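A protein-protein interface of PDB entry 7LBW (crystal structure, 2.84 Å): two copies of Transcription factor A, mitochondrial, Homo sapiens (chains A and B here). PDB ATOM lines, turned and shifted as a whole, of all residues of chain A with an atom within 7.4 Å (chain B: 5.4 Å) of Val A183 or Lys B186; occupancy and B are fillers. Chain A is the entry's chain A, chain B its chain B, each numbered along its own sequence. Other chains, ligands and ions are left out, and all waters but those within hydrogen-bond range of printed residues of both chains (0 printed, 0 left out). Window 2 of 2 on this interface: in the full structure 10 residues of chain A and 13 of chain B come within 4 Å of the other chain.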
ATOM      1  N   LEU A 110     -18.504 -22.513  10.906  1.00  0.00           N
ATOM      2  CA  LEU A 110     -18.322 -21.092  10.569  1.00  0.00           C
ATOM      3  C   LEU A 110     -19.235 -20.153  11.426  1.00  0.00           C
ATOM      4  O   LEU A 110     -19.126 -18.928  11.303  1.00  0.00           O
ATOM      5  CB  LEU A 110     -18.585 -20.880   9.072  1.00  0.00           C
ATOM      6  CG  LEU A 110     -17.610 -21.620   8.163  1.00  0.00           C
ATOM      7  CD1 LEU A 110     -18.038 -21.534   6.704  1.00  0.00           C
ATOM      8  CD2 LEU A 110     -16.196 -21.093   8.351  1.00  0.00           C
ATOM      9  N   GLU A 177     -21.591 -12.191   7.373  1.00  0.00           N
ATOM     10  CA  GLU A 177     -21.275 -12.005   5.964  1.00  0.00           C
ATOM     11  C   GLU A 177     -20.048 -11.126   5.761  1.00  0.00           C
ATOM     12  O   GLU A 177     -19.260 -11.398   4.868  1.00  0.00           O
ATOM     13  CB  GLU A 177     -22.494 -11.492   5.185  1.00  0.00           C
ATOM     14  CG  GLU A 177     -23.593 -12.539   5.041  1.00  0.00           C
ATOM     15  CD  GLU A 177     -24.694 -12.196   4.056  1.00  0.00           C
ATOM     16  OE1 GLU A 177     -24.965 -10.988   3.863  1.00  0.00           O
ATOM     17  OE2 GLU A 177     -25.352 -13.133   3.546  1.00  0.00           O
ATOM     18  N   GLU A 178     -19.826 -10.116   6.611  1.00  0.00           N
ATOM     19  CA  GLU A 178     -18.582  -9.326   6.532  1.00  0.00           C
ATOM     20  C   GLU A 178     -17.380 -10.238   6.826  1.00  0.00           C
ATOM     21  O   GLU A 178     -16.394 -10.205   6.111  1.00  0.00           O
ATOM     22  CB  GLU A 178     -18.610  -8.161   7.511  1.00  0.00           C
ATOM     23  CG  GLU A 178     -17.321  -7.372   7.556  1.00  0.00           C
ATOM     24  CD  GLU A 178     -17.425  -6.138   8.426  1.00  0.00           C
ATOM     25  OE1 GLU A 178     -17.281  -5.021   7.881  1.00  0.00           O
ATOM     26  OE2 GLU A 178     -17.697  -6.282   9.642  1.00  0.00           O
ATOM     27  N   GLN A 179     -17.515 -11.102   7.826  1.00  0.00           N
ATOM     28  CA  GLN A 179     -16.483 -12.038   8.219  1.00  0.00           C
ATOM     29  C   GLN A 179     -16.192 -13.091   7.144  1.00  0.00           C
ATOM     30  O   GLN A 179     -15.056 -13.538   7.041  1.00  0.00           O
ATOM     31  CB  GLN A 179     -16.849 -12.706   9.567  1.00  0.00           C
ATOM     32  CG  GLN A 179     -15.635 -12.885  10.507  1.00  0.00           C
ATOM     33  CD  GLN A 179     -15.770 -14.060  11.466  1.00  0.00           C
ATOM     34  OE1 GLN A 179     -16.877 -14.448  11.877  1.00  0.00           O
ATOM     35  NE2 GLN A 179     -14.638 -14.653  11.855  1.00  0.00           N
ATOM     36  N   MET A 180     -17.210 -13.522   6.371  1.00  0.00           N
ATOM     37  CA  MET A 180     -17.021 -14.536   5.311  1.00  0.00           C
ATOM     38  C   MET A 180     -16.238 -13.930   4.146  1.00  0.00           C
ATOM     39  O   MET A 180     -15.324 -14.577   3.644  1.00  0.00           O
ATOM     40  CB  MET A 180     -18.350 -15.100   4.826  1.00  0.00           C
ATOM     41  CG  MET A 180     -19.092 -15.875   5.876  1.00  0.00           C
ATOM     42  SD  MET A 180     -18.182 -17.292   6.513  1.00  0.00           S
ATOM     43  CE  MET A 180     -17.431 -16.610   7.999  1.00  0.00           C
ATOM     44  N   ILE A 181     -16.507 -12.677   3.764  1.00  0.00           N
ATOM     45  CA  ILE A 181     -15.686 -12.078   2.720  1.00  0.00           C
ATOM     46  C   ILE A 181     -14.176 -12.114   3.159  1.00  0.00           C
ATOM     47  O   ILE A 181     -13.306 -12.463   2.356  1.00  0.00           O
ATOM     48  CB  ILE A 181     -16.165 -10.651   2.393  1.00  0.00           C
ATOM     49  CG1 ILE A 181     -17.538 -10.680   1.698  1.00  0.00           C
ATOM     50  CG2 ILE A 181     -15.136  -9.952   1.508  1.00  0.00           C
ATOM     51  CD1 ILE A 181     -18.273  -9.431   1.847  1.00  0.00           C
ATOM     52  N   GLU A 182     -13.896 -11.820   4.452  1.00  0.00           N
ATOM     53  CA  GLU A 182     -12.539 -11.813   5.015  1.00  0.00           C
ATOM     54  C   GLU A 182     -11.891 -13.167   5.065  1.00  0.00           C
ATOM     55  O   GLU A 182     -10.706 -13.260   4.785  1.00  0.00           O
ATOM     56  CB  GLU A 182     -12.543 -11.222   6.410  1.00  0.00           C
ATOM     57  CG  GLU A 182     -12.757  -9.724   6.384  1.00  0.00           C
ATOM     58  CD  GLU A 182     -12.742  -9.089   7.751  1.00  0.00           C
ATOM     59  OE1 GLU A 182     -12.195  -9.710   8.688  1.00  0.00           O
ATOM     60  OE2 GLU A 182     -13.311  -7.986   7.893  1.00  0.00           O
ATOM     61  N   VAL A 183     -12.652 -14.210   5.408  1.00  0.00           N
ATOM     62  CA  VAL A 183     -12.170 -15.586   5.432  1.00  0.00           C
ATOM     63  C   VAL A 183     -12.018 -16.140   3.979  1.00  0.00           C
ATOM     64  O   VAL A 183     -11.429 -17.192   3.771  1.00  0.00           O
ATOM     65  CB  VAL A 183     -13.111 -16.413   6.349  1.00  0.00           C
ATOM     66  CG1 VAL A 183     -13.022 -17.917   6.099  1.00  0.00           C
ATOM     67  CG2 VAL A 183     -12.800 -16.112   7.812  1.00  0.00           C
ATOM     68  N   GLY A 184     -12.508 -15.399   2.993  1.00  0.00           N
ATOM     69  CA  GLY A 184     -12.420 -15.727   1.580  1.00  0.00           C
ATOM     70  C   GLY A 184     -13.537 -16.645   1.121  1.00  0.00           C
ATOM     71  O   GLY A 184     -13.341 -17.443   0.207  1.00  0.00           O
ATOM     72  N   ARG A 185     -14.736 -16.505   1.720  1.00  0.00           N
ATOM     73  CA  ARG A 185     -15.905 -17.293   1.410  1.00  0.00           C
ATOM     74  C   ARG A 185     -17.047 -16.382   0.997  1.00  0.00           C
ATOM     75  O   ARG A 185     -18.133 -16.452   1.561  1.00  0.00           O
ATOM     76  CB  ARG A 185     -16.281 -18.135   2.623  1.00  0.00           C
ATOM     77  CG  ARG A 185     -15.196 -19.113   3.052  1.00  0.00           C
ATOM     78  CD  ARG A 185     -14.797 -20.105   1.983  1.00  0.00           C
ATOM     79  NE  ARG A 185     -15.961 -20.758   1.398  1.00  0.00           N
ATOM     80  CZ  ARG A 185     -16.576 -21.831   1.886  1.00  0.00           C
ATOM     81  NH1 ARG A 185     -16.124 -22.425   2.983  1.00  0.00           N
ATOM     82  NH2 ARG A 185     -17.646 -22.325   1.277  1.00  0.00           N
ATOM     83  N   LYS A 186     -16.802 -15.584  -0.049  1.00  0.00           N
ATOM     84  CA  LYS A 186     -17.780 -14.677  -0.638  1.00  0.00           C
ATOM     85  C   LYS A 186     -18.942 -15.478  -1.241  1.00  0.00           C
ATOM     86  O   LYS A 186     -20.006 -14.910  -1.448  1.00  0.00           O
ATOM     87  CB  LYS A 186     -17.112 -13.793  -1.701  1.00  0.00           C
ATOM     88  CG  LYS A 186     -17.867 -12.518  -2.029  1.00  0.00           C
ATOM     89  CD  LYS A 186     -17.039 -11.537  -2.892  1.00  0.00           C
ATOM     90  CE  LYS A 186     -15.949 -10.797  -2.142  1.00  0.00           C
ATOM     91  NZ  LYS A 186     -15.133  -9.914  -3.026  1.00  0.00           N
ATOM     92  N   ASP A 187     -18.738 -16.788  -1.539  1.00  0.00           N
ATOM     93  CA  ASP A 187     -19.761 -17.722  -2.019  1.00  0.00           C
ATOM     94  C   ASP A 187     -20.884 -17.977  -1.007  1.00  0.00           C
ATOM     95  O   ASP A 187     -21.992 -18.316  -1.419  1.00  0.00           O
ATOM     96  CB  ASP A 187     -19.126 -19.082  -2.391  1.00  0.00           C
ATOM     97  CG  ASP A 187     -18.457 -19.807  -1.235  1.00  0.00           C
ATOM     98  OD1 ASP A 187     -17.473 -19.260  -0.678  1.00  0.00           O
ATOM     99  OD2 ASP A 187     -18.885 -20.945  -0.911  1.00  0.00           O
ATOM    100  N   LEU A 188     -20.605 -17.874   0.302  1.00  0.00           N
ATOM    101  CA  LEU A 188     -21.597 -18.138   1.348  1.00  0.00           C
ATOM    102  C   LEU A 188     -22.556 -16.960   1.554  1.00  0.00           C
ATOM    103  O   LEU A 188     -23.467 -17.081   2.383  1.00  0.00           O
ATOM    104  CB  LEU A 188     -20.882 -18.500   2.668  1.00  0.00           C
ATOM    105  CG  LEU A 188     -19.959 -19.724   2.629  1.00  0.00           C
ATOM    106  CD1 LEU A 188     -19.298 -19.946   3.953  1.00  0.00           C
ATOM    107  CD2 LEU A 188     -20.708 -20.954   2.222  1.00  0.00           C
ATOM    108  N   MET B 180      -7.499 -15.858  -6.449  1.00  0.00           N
ATOM    109  CA  MET B 180      -8.835 -16.185  -5.972  1.00  0.00           C
ATOM    110  C   MET B 180      -8.973 -15.882  -4.485  1.00  0.00           C
ATOM    111  O   MET B 180     -10.038 -15.415  -4.107  1.00  0.00           O
ATOM    112  CB  MET B 180      -9.209 -17.628  -6.324  1.00  0.00           C
ATOM    113  CG  MET B 180      -9.370 -17.830  -7.793  1.00  0.00           C
ATOM    114  SD  MET B 180     -10.691 -16.834  -8.517  1.00  0.00           S
ATOM    115  CE  MET B 180      -9.793 -15.535  -9.330  1.00  0.00           C
ATOM    116  N   ILE B 181      -7.893 -16.026  -3.667  1.00  0.00           N
ATOM    117  CA  ILE B 181      -7.906 -15.610  -2.258  1.00  0.00           C
ATOM    118  C   ILE B 181      -8.087 -14.079  -2.202  1.00  0.00           C
ATOM    119  O   ILE B 181      -8.834 -13.608  -1.336  1.00  0.00           O
ATOM    120  CB  ILE B 181      -6.644 -16.039  -1.452  1.00  0.00           C
ATOM    121  CG1 ILE B 181      -6.557 -17.568  -1.307  1.00  0.00           C
ATOM    122  CG2 ILE B 181      -6.668 -15.397  -0.061  1.00  0.00           C
ATOM    123  CD1 ILE B 181      -5.230 -18.078  -0.894  1.00  0.00           C
ATOM    124  N   GLY B 184     -11.571 -13.220  -2.667  1.00  0.00           N
ATOM    125  CA  GLY B 184     -12.352 -13.807  -1.589  1.00  0.00           C
ATOM    126  C   GLY B 184     -13.090 -15.063  -1.993  1.00  0.00           C
ATOM    127  O   GLY B 184     -14.204 -15.302  -1.521  1.00  0.00           O
ATOM    128  N   ARG B 185     -12.453 -15.891  -2.847  1.00  0.00           N
ATOM    129  CA  ARG B 185     -13.003 -17.131  -3.348  1.00  0.00           C
ATOM    130  C   ARG B 185     -12.071 -18.298  -3.001  1.00  0.00           C
ATOM    131  O   ARG B 185     -11.685 -19.038  -3.894  1.00  0.00           O
ATOM    132  CB  ARG B 185     -13.207 -17.012  -4.865  1.00  0.00           C
ATOM    133  CG  ARG B 185     -14.162 -15.904  -5.284  1.00  0.00           C
ATOM    134  CD  ARG B 185     -15.549 -16.040  -4.702  1.00  0.00           C
ATOM    135  NE  ARG B 185     -16.089 -17.379  -4.911  1.00  0.00           N
ATOM    136  CZ  ARG B 185     -16.718 -17.797  -6.008  1.00  0.00           C
ATOM    137  NH1 ARG B 185     -16.929 -16.965  -7.027  1.00  0.00           N
ATOM    138  NH2 ARG B 185     -17.152 -19.049  -6.093  1.00  0.00           N
ATOM    139  N   LYS B 186     -11.730 -18.511  -1.699  1.00  0.00           N
ATOM    140  CA  LYS B 186     -10.926 -19.677  -1.232  1.00  0.00           C
ATOM    141  C   LYS B 186     -11.673 -20.978  -1.579  1.00  0.00           C
ATOM    142  O   LYS B 186     -11.040 -22.030  -1.693  1.00  0.00           O
ATOM    143  CB  LYS B 186     -10.693 -19.693   0.308  1.00  0.00           C
ATOM    144  CG  LYS B 186      -9.410 -19.045   0.818  1.00  0.00           C
ATOM    145  CD  LYS B 186      -9.183 -19.381   2.314  1.00  0.00           C
ATOM    146  CE  LYS B 186      -7.999 -18.688   2.984  1.00  0.00           C
ATOM    147  NZ  LYS B 186      -8.266 -17.264   3.304  1.00  0.00           N
ATOM    148  N   ASP B 187     -13.026 -20.922  -1.709  1.00  0.00           N
ATOM    149  CA  ASP B 187     -13.823 -22.092  -2.079  1.00  0.00           C
ATOM    150  C   ASP B 187     -13.407 -22.707  -3.421  1.00  0.00           C
ATOM    151  O   ASP B 187     -13.641 -23.900  -3.637  1.00  0.00           O
ATOM    152  CB  ASP B 187     -15.316 -21.738  -2.155  1.00  0.00           C
ATOM    153  CG  ASP B 187     -15.673 -20.689  -3.196  1.00  0.00           C
ATOM    154  OD1 ASP B 187     -15.197 -19.534  -3.064  1.00  0.00           O
ATOM    155  OD2 ASP B 187     -16.464 -21.013  -4.128  1.00  0.00           O
ATOM    156  N   LEU B 188     -12.851 -21.889  -4.344  1.00  0.00           N
ATOM    157  CA  LEU B 188     -12.447 -22.364  -5.664  1.00  0.00           C
ATOM    158  C   LEU B 188     -11.084 -23.076  -5.648  1.00  0.00           C
ATOM    159  O   LEU B 188     -10.677 -23.577  -6.688  1.00  0.00           O
ATOM    160  CB  LEU B 188     -12.430 -21.189  -6.667  1.00  0.00           C
ATOM    161  CG  LEU B 188     -13.752 -20.444  -6.861  1.00  0.00           C
ATOM    162  CD1 LEU B 188     -13.597 -19.313  -7.825  1.00  0.00           C
ATOM    163  CD2 LEU B 188     -14.833 -21.362  -7.327  1.00  0.00           C
ATOM    164  N   LEU B 189     -10.383 -23.140  -4.504  1.00  0.00           N
ATOM    165  CA  LEU B 189      -9.076 -23.795  -4.431  1.00  0.00           C
ATOM    166  C   LEU B 189      -9.189 -25.303  -4.273  1.00  0.00           C
ATOM    167  O   LEU B 189     -10.222 -25.809  -3.846  1.00  0.00           O
ATOM    168  CB  LEU B 189      -8.248 -23.211  -3.275  1.00  0.00           C
ATOM    169  CG  LEU B 189      -7.576 -21.877  -3.527  1.00  0.00           C
ATOM    170  CD1 LEU B 189      -8.399 -20.931  -4.420  1.00  0.00           C
ATOM    171  CD2 LEU B 189      -7.209 -21.226  -2.232  1.00  0.00           C
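Printed residues of chain B that touch a printed residue of chain A: Gly B184, Arg B185, Lys B186 and Asp B187. Along chain B the printed residues that touch a printed residue of chain A span positions 184 to 187. Among the printed residues, no Asp or Glu carboxylate lies within 4 Å of a Lys or Arg side-chain nitrogen of the other chain.
O of Val A183 is in hydrogen-bond range of NZ of Lys B186 (3.2 Å). The backbone carbonyl oxygen (O) of Gly B184 is in hydrogen-bond range of the backbone NH (N) of Lys A186 (3.0 Å). O of Gly B184 lies within hydrogen-bond range of N of Arg A185 (3.5 Å). The backbone carbonyl oxygen (O) of Gly A184 sits close to the backbone carbonyl oxygen (O) of Gly B184. The backbone carbonyl oxygen of Gly A184 is in hydrogen-bond range of the backbone NH of Lys B186 (2.7 Å). The side-chain carboxylate (OD1) of Asp A187 lies close to the side-chain carboxylate (OD1) of Asp B187, at 3.3 Å.
Printed residues of chain B within 4 Å of Val A183: Lys B186 (3.2 Å). Printed residues of chain B within 4 Å of Arg A185: Gly B184 (3.5 Å) and Asp B187 (3.7 Å). Printed residues of chain A within 4 Å of Gly B184: Gly A184 (2.9 Å), Arg A185 (3.5 Å) and Lys A186 (3.0 Å). Lys B186 touches just these residues of chain A: Val A183 and Gly A184. Leu B188 touches none of the printed residues of chain A. The nearest printed residue of chain B that does not touch Val A183 is Gly B184 (6.0 Å). The nearest residue of chain A that does not touch Lys B186 is Arg A185 (4.5 Å).
Gly A184 touches its own counterpart, Gly B184. Gly A184 touches Arg B185, and with the chains exchanged Arg A185 touches Gly B184. Gly A184 touches Asp B187, but with the chains exchanged Asp A187 does not touch Gly B184 (4.8 Å). Arg A185 touches Asp B187, but with the chains exchanged Asp A187 does not touch Arg B185 (4.2 Å). 7 positions are printed for both chains. Of the 9 pairs that touch across the chains among the printed residues, 6 have their exchanged pair printed and touching as well.
Gly A184 touches Arg B185. Asp B187 touches Gly A184. Arg A185 touches Asp B187.
O of Met A180 is in hydrogen-bond range of N of Arg A185, at 2.8 Å. NH2 of Arg A185 lies within salt-bridge range of OD2 of Asp A187 (2.9 Å). The side-chain carboxylate of Asp B187 lies within salt-bridge range of the guanidinium group of Arg B185 (2.9 Å). The backbone NH of Arg B185 is in hydrogen-bond range of the backbone carbonyl oxygen of Met B180.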
